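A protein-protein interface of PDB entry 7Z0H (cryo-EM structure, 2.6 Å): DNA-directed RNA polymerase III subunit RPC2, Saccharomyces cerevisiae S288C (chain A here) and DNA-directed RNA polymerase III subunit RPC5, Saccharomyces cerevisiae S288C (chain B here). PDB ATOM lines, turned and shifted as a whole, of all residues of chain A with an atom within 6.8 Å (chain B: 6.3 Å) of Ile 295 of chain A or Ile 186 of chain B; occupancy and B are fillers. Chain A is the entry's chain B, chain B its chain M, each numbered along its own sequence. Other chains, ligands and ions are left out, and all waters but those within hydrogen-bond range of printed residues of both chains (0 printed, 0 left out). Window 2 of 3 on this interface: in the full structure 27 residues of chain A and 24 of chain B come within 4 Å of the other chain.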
ATOM      1  N   LYS A 258      14.461   1.410  24.628  1.00  0.00           N
ATOM      2  CA  LYS A 258      13.431   0.838  23.767  1.00  0.00           C
ATOM      3  C   LYS A 258      12.405   1.888  23.362  1.00  0.00           C
ATOM      4  O   LYS A 258      11.892   1.865  22.237  1.00  0.00           O
ATOM      5  CB  LYS A 258      12.756  -0.338  24.473  1.00  0.00           C
ATOM      6  CG  LYS A 258      13.467  -1.663  24.258  1.00  0.00           C
ATOM      7  CD  LYS A 258      12.642  -2.830  24.762  1.00  0.00           C
ATOM      8  CE  LYS A 258      13.360  -4.148  24.527  1.00  0.00           C
ATOM      9  NZ  LYS A 258      13.576  -4.412  23.080  1.00  0.00           N
ATOM     10  N   ASP A 265      17.351  -4.958  21.760  1.00  0.00           N
ATOM     11  CA  ASP A 265      17.822  -5.398  23.073  1.00  0.00           C
ATOM     12  C   ASP A 265      19.143  -6.151  22.981  1.00  0.00           C
ATOM     13  O   ASP A 265      19.748  -6.479  24.007  1.00  0.00           O
ATOM     14  CB  ASP A 265      16.770  -6.251  23.786  1.00  0.00           C
ATOM     15  CG  ASP A 265      17.012  -6.350  25.278  1.00  0.00           C
ATOM     16  OD1 ASP A 265      16.842  -5.331  25.979  1.00  0.00           O
ATOM     17  OD2 ASP A 265      17.369  -7.450  25.749  1.00  0.00           O
ATOM     18  N   SER A 290      14.497  -5.428  32.026  1.00  0.00           N
ATOM     19  CA  SER A 290      13.648  -5.045  30.904  1.00  0.00           C
ATOM     20  C   SER A 290      12.561  -6.085  30.665  1.00  0.00           C
ATOM     21  O   SER A 290      11.408  -5.734  30.389  1.00  0.00           O
ATOM     22  CB  SER A 290      14.494  -4.850  29.647  1.00  0.00           C
ATOM     23  OG  SER A 290      13.688  -4.853  28.483  1.00  0.00           O
ATOM     24  N   SER A 291      12.905  -7.366  30.766  1.00  0.00           N
ATOM     25  CA  SER A 291      11.926  -8.429  30.600  1.00  0.00           C
ATOM     26  C   SER A 291      11.289  -8.869  31.910  1.00  0.00           C
ATOM     27  O   SER A 291      10.245  -9.530  31.881  1.00  0.00           O
ATOM     28  CB  SER A 291      12.572  -9.644  29.931  1.00  0.00           C
ATOM     29  OG  SER A 291      11.921 -10.833  30.336  1.00  0.00           O
ATOM     30  N   LYS A 292      11.890  -8.518  33.050  1.00  0.00           N
ATOM     31  CA  LYS A 292      11.371  -8.967  34.339  1.00  0.00           C
ATOM     32  C   LYS A 292       9.949  -8.476  34.562  1.00  0.00           C
ATOM     33  O   LYS A 292       9.108  -9.207  35.099  1.00  0.00           O
ATOM     34  CB  LYS A 292      12.290  -8.493  35.464  1.00  0.00           C
ATOM     35  CG  LYS A 292      12.174  -9.298  36.746  1.00  0.00           C
ATOM     36  CD  LYS A 292      12.749  -8.539  37.929  1.00  0.00           C
ATOM     37  CE  LYS A 292      14.171  -8.077  37.647  1.00  0.00           C
ATOM     38  NZ  LYS A 292      14.717  -7.249  38.754  1.00  0.00           N
ATOM     39  N   LEU A 293       9.661  -7.240  34.163  1.00  0.00           N
ATOM     40  CA  LEU A 293       8.299  -6.731  34.212  1.00  0.00           C
ATOM     41  C   LEU A 293       7.456  -7.451  33.169  1.00  0.00           C
ATOM     42  O   LEU A 293       6.495  -8.151  33.507  1.00  0.00           O
ATOM     43  CB  LEU A 293       8.292  -5.220  33.978  1.00  0.00           C
ATOM     44  CG  LEU A 293       9.317  -4.450  34.815  1.00  0.00           C
ATOM     45  CD1 LEU A 293       9.169  -2.962  34.608  1.00  0.00           C
ATOM     46  CD2 LEU A 293       9.176  -4.793  36.292  1.00  0.00           C
ATOM     47  N   ASP A 294       7.830  -7.292  31.902  1.00  0.00           N
ATOM     48  CA  ASP A 294       7.223  -7.981  30.769  1.00  0.00           C
ATOM     49  C   ASP A 294       8.039  -7.636  29.533  1.00  0.00           C
ATOM     50  O   ASP A 294       8.706  -6.599  29.483  1.00  0.00           O
ATOM     51  CB  ASP A 294       5.754  -7.592  30.572  1.00  0.00           C
ATOM     52  CG  ASP A 294       5.520  -6.107  30.738  1.00  0.00           C
ATOM     53  OD1 ASP A 294       6.465  -5.403  31.146  1.00  0.00           O
ATOM     54  OD2 ASP A 294       4.396  -5.642  30.456  1.00  0.00           O
ATOM     55  N   ILE A 295       7.981  -8.517  28.536  1.00  0.00           N
ATOM     56  CA  ILE A 295       8.705  -8.263  27.299  1.00  0.00           C
ATOM     57  C   ILE A 295       8.039  -7.113  26.548  1.00  0.00           C
ATOM     58  O   ILE A 295       6.857  -6.812  26.734  1.00  0.00           O
ATOM     59  CB  ILE A 295       8.802  -9.528  26.432  1.00  0.00           C
ATOM     60  CG1 ILE A 295      10.098  -9.495  25.620  1.00  0.00           C
ATOM     61  CG2 ILE A 295       7.580  -9.664  25.535  1.00  0.00           C
ATOM     62  CD1 ILE A 295      11.346  -9.443  26.468  1.00  0.00           C
ATOM     63  N   TYR A 296       8.816  -6.455  25.692  1.00  0.00           N
ATOM     64  CA  TYR A 296       8.502  -5.095  25.283  1.00  0.00           C
ATOM     65  C   TYR A 296       8.551  -4.895  23.779  1.00  0.00           C
ATOM     66  O   TYR A 296       9.460  -5.378  23.097  1.00  0.00           O
ATOM     67  CB  TYR A 296       9.468  -4.122  25.948  1.00  0.00           C
ATOM     68  CG  TYR A 296       9.099  -3.817  27.369  1.00  0.00           C
ATOM     69  CD1 TYR A 296       7.770  -3.763  27.761  1.00  0.00           C
ATOM     70  CD2 TYR A 296      10.073  -3.637  28.331  1.00  0.00           C
ATOM     71  CE1 TYR A 296       7.425  -3.493  29.061  1.00  0.00           C
ATOM     72  CE2 TYR A 296       9.737  -3.378  29.634  1.00  0.00           C
ATOM     73  CZ  TYR A 296       8.414  -3.305  29.998  1.00  0.00           C
ATOM     74  OH  TYR A 296       8.085  -3.043  31.307  1.00  0.00           O
ATOM     75  N   THR A 297       7.559  -4.167  23.281  1.00  0.00           N
ATOM     76  CA  THR A 297       7.635  -3.461  22.018  1.00  0.00           C
ATOM     77  C   THR A 297       8.088  -2.035  22.309  1.00  0.00           C
ATOM     78  O   THR A 297       8.283  -1.647  23.464  1.00  0.00           O
ATOM     79  CB  THR A 297       6.281  -3.473  21.306  1.00  0.00           C
ATOM     80  OG1 THR A 297       5.360  -2.643  22.024  1.00  0.00           O
ATOM     81  CG2 THR A 297       5.725  -4.879  21.266  1.00  0.00           C
ATOM     82  N   GLN A 300       4.991  -0.238  24.073  1.00  0.00           N
ATOM     83  CA  GLN A 300       4.782  -0.610  25.470  1.00  0.00           C
ATOM     84  C   GLN A 300       5.677   0.200  26.402  1.00  0.00           C
ATOM     85  O   GLN A 300       5.207   0.740  27.412  1.00  0.00           O
ATOM     86  CB  GLN A 300       5.033  -2.105  25.661  1.00  0.00           C
ATOM     87  CG  GLN A 300       3.784  -2.910  25.975  1.00  0.00           C
ATOM     88  CD  GLN A 300       4.087  -4.124  26.831  1.00  0.00           C
ATOM     89  OE1 GLN A 300       4.571  -5.142  26.336  1.00  0.00           O
ATOM     90  NE2 GLN A 300       3.810  -4.020  28.126  1.00  0.00           N
ATOM     91  N   TRP B 140      -0.230 -15.364  21.356  1.00  0.00           N
ATOM     92  CA  TRP B 140      -0.591 -14.381  20.341  1.00  0.00           C
ATOM     93  C   TRP B 140      -1.107 -15.101  19.102  1.00  0.00           C
ATOM     94  O   TRP B 140      -0.442 -16.001  18.583  1.00  0.00           O
ATOM     95  CB  TRP B 140       0.608 -13.494  19.988  1.00  0.00           C
ATOM     96  CG  TRP B 140       1.282 -12.914  21.196  1.00  0.00           C
ATOM     97  CD1 TRP B 140       0.741 -12.042  22.094  1.00  0.00           C
ATOM     98  CD2 TRP B 140       2.615 -13.179  21.646  1.00  0.00           C
ATOM     99  NE1 TRP B 140       1.655 -11.741  23.072  1.00  0.00           N
ATOM    100  CE2 TRP B 140       2.815 -12.426  22.821  1.00  0.00           C
ATOM    101  CE3 TRP B 140       3.659 -13.975  21.171  1.00  0.00           C
ATOM    102  CZ2 TRP B 140       4.016 -12.447  23.524  1.00  0.00           C
ATOM    103  CZ3 TRP B 140       4.850 -13.993  21.869  1.00  0.00           C
ATOM    104  CH2 TRP B 140       5.018 -13.235  23.034  1.00  0.00           C
ATOM    105  N   PHE B 183       6.598  -6.279  16.946  1.00  0.00           N
ATOM    106  CA  PHE B 183       5.778  -7.262  17.647  1.00  0.00           C
ATOM    107  C   PHE B 183       4.321  -6.818  17.697  1.00  0.00           C
ATOM    108  O   PHE B 183       3.712  -6.737  18.774  1.00  0.00           O
ATOM    109  CB  PHE B 183       6.326  -7.519  19.052  1.00  0.00           C
ATOM    110  CG  PHE B 183       7.826  -7.487  19.135  1.00  0.00           C
ATOM    111  CD1 PHE B 183       8.576  -8.577  18.730  1.00  0.00           C
ATOM    112  CD2 PHE B 183       8.487  -6.373  19.626  1.00  0.00           C
ATOM    113  CE1 PHE B 183       9.953  -8.556  18.807  1.00  0.00           C
ATOM    114  CE2 PHE B 183       9.865  -6.346  19.704  1.00  0.00           C
ATOM    115  CZ  PHE B 183      10.599  -7.441  19.293  1.00  0.00           C
ATOM    116  N   LYS B 184       3.777  -6.488  16.526  1.00  0.00           N
ATOM    117  CA  LYS B 184       2.375  -6.129  16.350  1.00  0.00           C
ATOM    118  C   LYS B 184       1.434  -7.105  17.044  1.00  0.00           C
ATOM    119  O   LYS B 184       0.375  -6.701  17.529  1.00  0.00           O
ATOM    120  CB  LYS B 184       2.034  -6.060  14.860  1.00  0.00           C
ATOM    121  CG  LYS B 184       3.049  -6.746  13.963  1.00  0.00           C
ATOM    122  CD  LYS B 184       2.639  -6.666  12.503  1.00  0.00           C
ATOM    123  CE  LYS B 184       2.763  -5.251  11.968  1.00  0.00           C
ATOM    124  NZ  LYS B 184       2.292  -5.160  10.558  1.00  0.00           N
ATOM    125  N   TYR B 185       1.791  -8.392  17.080  1.00  0.00           N
ATOM    126  CA  TYR B 185       0.957  -9.354  17.794  1.00  0.00           C
ATOM    127  C   TYR B 185       0.928  -9.058  19.289  1.00  0.00           C
ATOM    128  O   TYR B 185      -0.132  -9.134  19.923  1.00  0.00           O
ATOM    129  CB  TYR B 185       1.435 -10.783  17.527  1.00  0.00           C
ATOM    130  CG  TYR B 185       2.932 -10.993  17.580  1.00  0.00           C
ATOM    131  CD1 TYR B 185       3.713 -10.860  16.438  1.00  0.00           C
ATOM    132  CD2 TYR B 185       3.561 -11.359  18.763  1.00  0.00           C
ATOM    133  CE1 TYR B 185       5.078 -11.066  16.478  1.00  0.00           C
ATOM    134  CE2 TYR B 185       4.928 -11.566  18.813  1.00  0.00           C
ATOM    135  CZ  TYR B 185       5.680 -11.419  17.668  1.00  0.00           C
ATOM    136  OH  TYR B 185       7.040 -11.624  17.709  1.00  0.00           O
ATOM    137  N   ILE B 186       2.080  -8.714  19.870  1.00  0.00           N
ATOM    138  CA  ILE B 186       2.106  -8.295  21.268  1.00  0.00           C
ATOM    139  C   ILE B 186       1.294  -7.023  21.454  1.00  0.00           C
ATOM    140  O   ILE B 186       0.577  -6.867  22.450  1.00  0.00           O
ATOM    141  CB  ILE B 186       3.554  -8.102  21.749  1.00  0.00           C
ATOM    142  CG1 ILE B 186       4.321  -9.414  21.690  1.00  0.00           C
ATOM    143  CG2 ILE B 186       3.581  -7.557  23.168  1.00  0.00           C
ATOM    144  CD1 ILE B 186       5.691  -9.288  22.262  1.00  0.00           C
ATOM    145  N   ASP B 187       1.409  -6.087  20.511  1.00  0.00           N
ATOM    146  CA  ASP B 187       0.622  -4.857  20.577  1.00  0.00           C
ATOM    147  C   ASP B 187      -0.871  -5.164  20.622  1.00  0.00           C
ATOM    148  O   ASP B 187      -1.614  -4.607  21.441  1.00  0.00           O
ATOM    149  CB  ASP B 187       0.955  -3.974  19.374  1.00  0.00           C
ATOM    150  CG  ASP B 187       0.589  -2.520  19.591  1.00  0.00           C
ATOM    151  OD1 ASP B 187      -0.245  -2.235  20.474  1.00  0.00           O
ATOM    152  OD2 ASP B 187       1.135  -1.660  18.869  1.00  0.00           O
ATOM    153  N   ASP B 188      -1.325  -6.057  19.739  1.00  0.00           N
ATOM    154  CA  ASP B 188      -2.739  -6.413  19.681  1.00  0.00           C
ATOM    155  C   ASP B 188      -3.183  -7.125  20.952  1.00  0.00           C
ATOM    156  O   ASP B 188      -4.271  -6.857  21.475  1.00  0.00           O
ATOM    157  CB  ASP B 188      -3.009  -7.287  18.457  1.00  0.00           C
ATOM    158  CG  ASP B 188      -3.034  -6.491  17.168  1.00  0.00           C
ATOM    159  OD1 ASP B 188      -2.712  -5.285  17.207  1.00  0.00           O
ATOM    160  OD2 ASP B 188      -3.376  -7.072  16.116  1.00  0.00           O
ATOM    161  N   ALA B 189      -2.358  -8.043  21.460  1.00  0.00           N
ATOM    162  CA  ALA B 189      -2.702  -8.726  22.703  1.00  0.00           C
ATOM    163  C   ALA B 189      -2.812  -7.738  23.856  1.00  0.00           C
ATOM    164  O   ALA B 189      -3.730  -7.830  24.679  1.00  0.00           O
ATOM    165  CB  ALA B 189      -1.667  -9.804  23.016  1.00  0.00           C
ATOM    166  N   ASN B 190      -1.896  -6.771  23.921  1.00  0.00           N
ATOM    167  CA  ASN B 190      -1.923  -5.800  25.007  1.00  0.00           C
ATOM    168  C   ASN B 190      -3.133  -4.878  24.902  1.00  0.00           C
ATOM    169  O   ASN B 190      -3.748  -4.545  25.921  1.00  0.00           O
ATOM    170  CB  ASN B 190      -0.623  -4.997  25.024  1.00  0.00           C
ATOM    171  CG  ASN B 190       0.555  -5.810  25.532  1.00  0.00           C
ATOM    172  OD1 ASN B 190       1.655  -5.741  24.984  1.00  0.00           O
ATOM    173  ND2 ASN B 190       0.326  -6.593  26.580  1.00  0.00           N
ATOM    174  N   VAL B 191      -3.497  -4.457  23.688  1.00  0.00           N
ATOM    175  CA  VAL B 191      -4.666  -3.589  23.552  1.00  0.00           C
ATOM    176  C   VAL B 191      -5.948  -4.361  23.860  1.00  0.00           C
ATOM    177  O   VAL B 191      -6.871  -3.828  24.490  1.00  0.00           O
ATOM    178  CB  VAL B 191      -4.703  -2.919  22.162  1.00  0.00           C
ATOM    179  CG1 VAL B 191      -5.044  -3.907  21.062  1.00  0.00           C
ATOM    180  CG2 VAL B 191      -5.692  -1.759  22.160  1.00  0.00           C
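The side-chain amide oxygen (OE1) of Gln 300 of chain A lies close to the side-chain amide oxygen (OD1) of Asn 190 of chain B, at 3.3 Å.
OH of Tyr 296 of chain A is in hydrogen-bond range of OD1 of Asp 294 of chain A (2.9 Å).
The backbone carbonyl oxygen of Ile 295 of chain A sits close to the side-chain amide oxygen of Gln 300 of chain A (2.9 Å).
The side-chain amide oxygen (OD1) of Asn 190 of chain B lies close to the backbone carbonyl oxygen (O) of Ile 186 of chain B, at 3.0 Å.
The side-chain carboxylate of Asp 294 of chain A lies within hydrogen-bond range of the side-chain amide nitrogen of Gln 300 of chain A (2.9 Å).
OG1 of Thr 297 of chain A lies within hydrogen-bond range of N of Gln 300 of chain A, at 3.2 Å.
Among the printed residues, merely in contact across the chains: Thr 297 of chain A with Phe 183 of chain B (3.5 Å), Tyr 296 of chain A with Phe 183 of chain B (3.6 Å), Ile 295 of chain A with Ile 186 of chain B (3.8 Å) and Thr 297 of chain A with Ile 186 of chain B (3.9 Å).
Of chain B, only Ile 186 (3.8 Å) comes within 4 Å of Ile 295 of chain A.
Of the printed residues of chain B, Tyr 296 of chain A touches Phe 183.
Printed residues of chain B within 4 Å of Thr 297 of chain A: Phe 183 (3.5 Å) and Ile 186 (3.9 Å).
Of the printed residues of chain B, Gln 300 of chain A touches Asn 190.
Printed residues of chain A within 4 Å of Phe 183 of chain B: Tyr 296 (3.6 Å) and Thr 297 (3.5 Å).
Of chain A, only Ile 295 and Thr 297 come within 4 Å of Ile 186 of chain B.
Of the printed residues of chain A, Asn 190 of chain B touches Gln 300.
Val 191 of chain B touches none of the printed residues of chain A.
The nearest residue of chain B that does not touch Ile 295 of chain A is Trp 140 of chain B (4.9 Å).
The nearest residue of chain A that does not touch Ile 186 of chain B is Gln 300 of chain A (4.1 Å).
Of the 11 printed residues of chain A, 4 touch a printed residue of chain B.
Printed residues of chain B that touch a printed residue of chain A: Phe 183, Ile 186 and Asn 190.
Hydrophobic or aromatic side chains of chain B within 4 Å of the printed part of chain A: Phe 183 and Ile 186.
Among the printed residues, no Asp or Glu carboxylate lies within 4 Å of a Lys or Arg side-chain nitrogen of the other chain.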
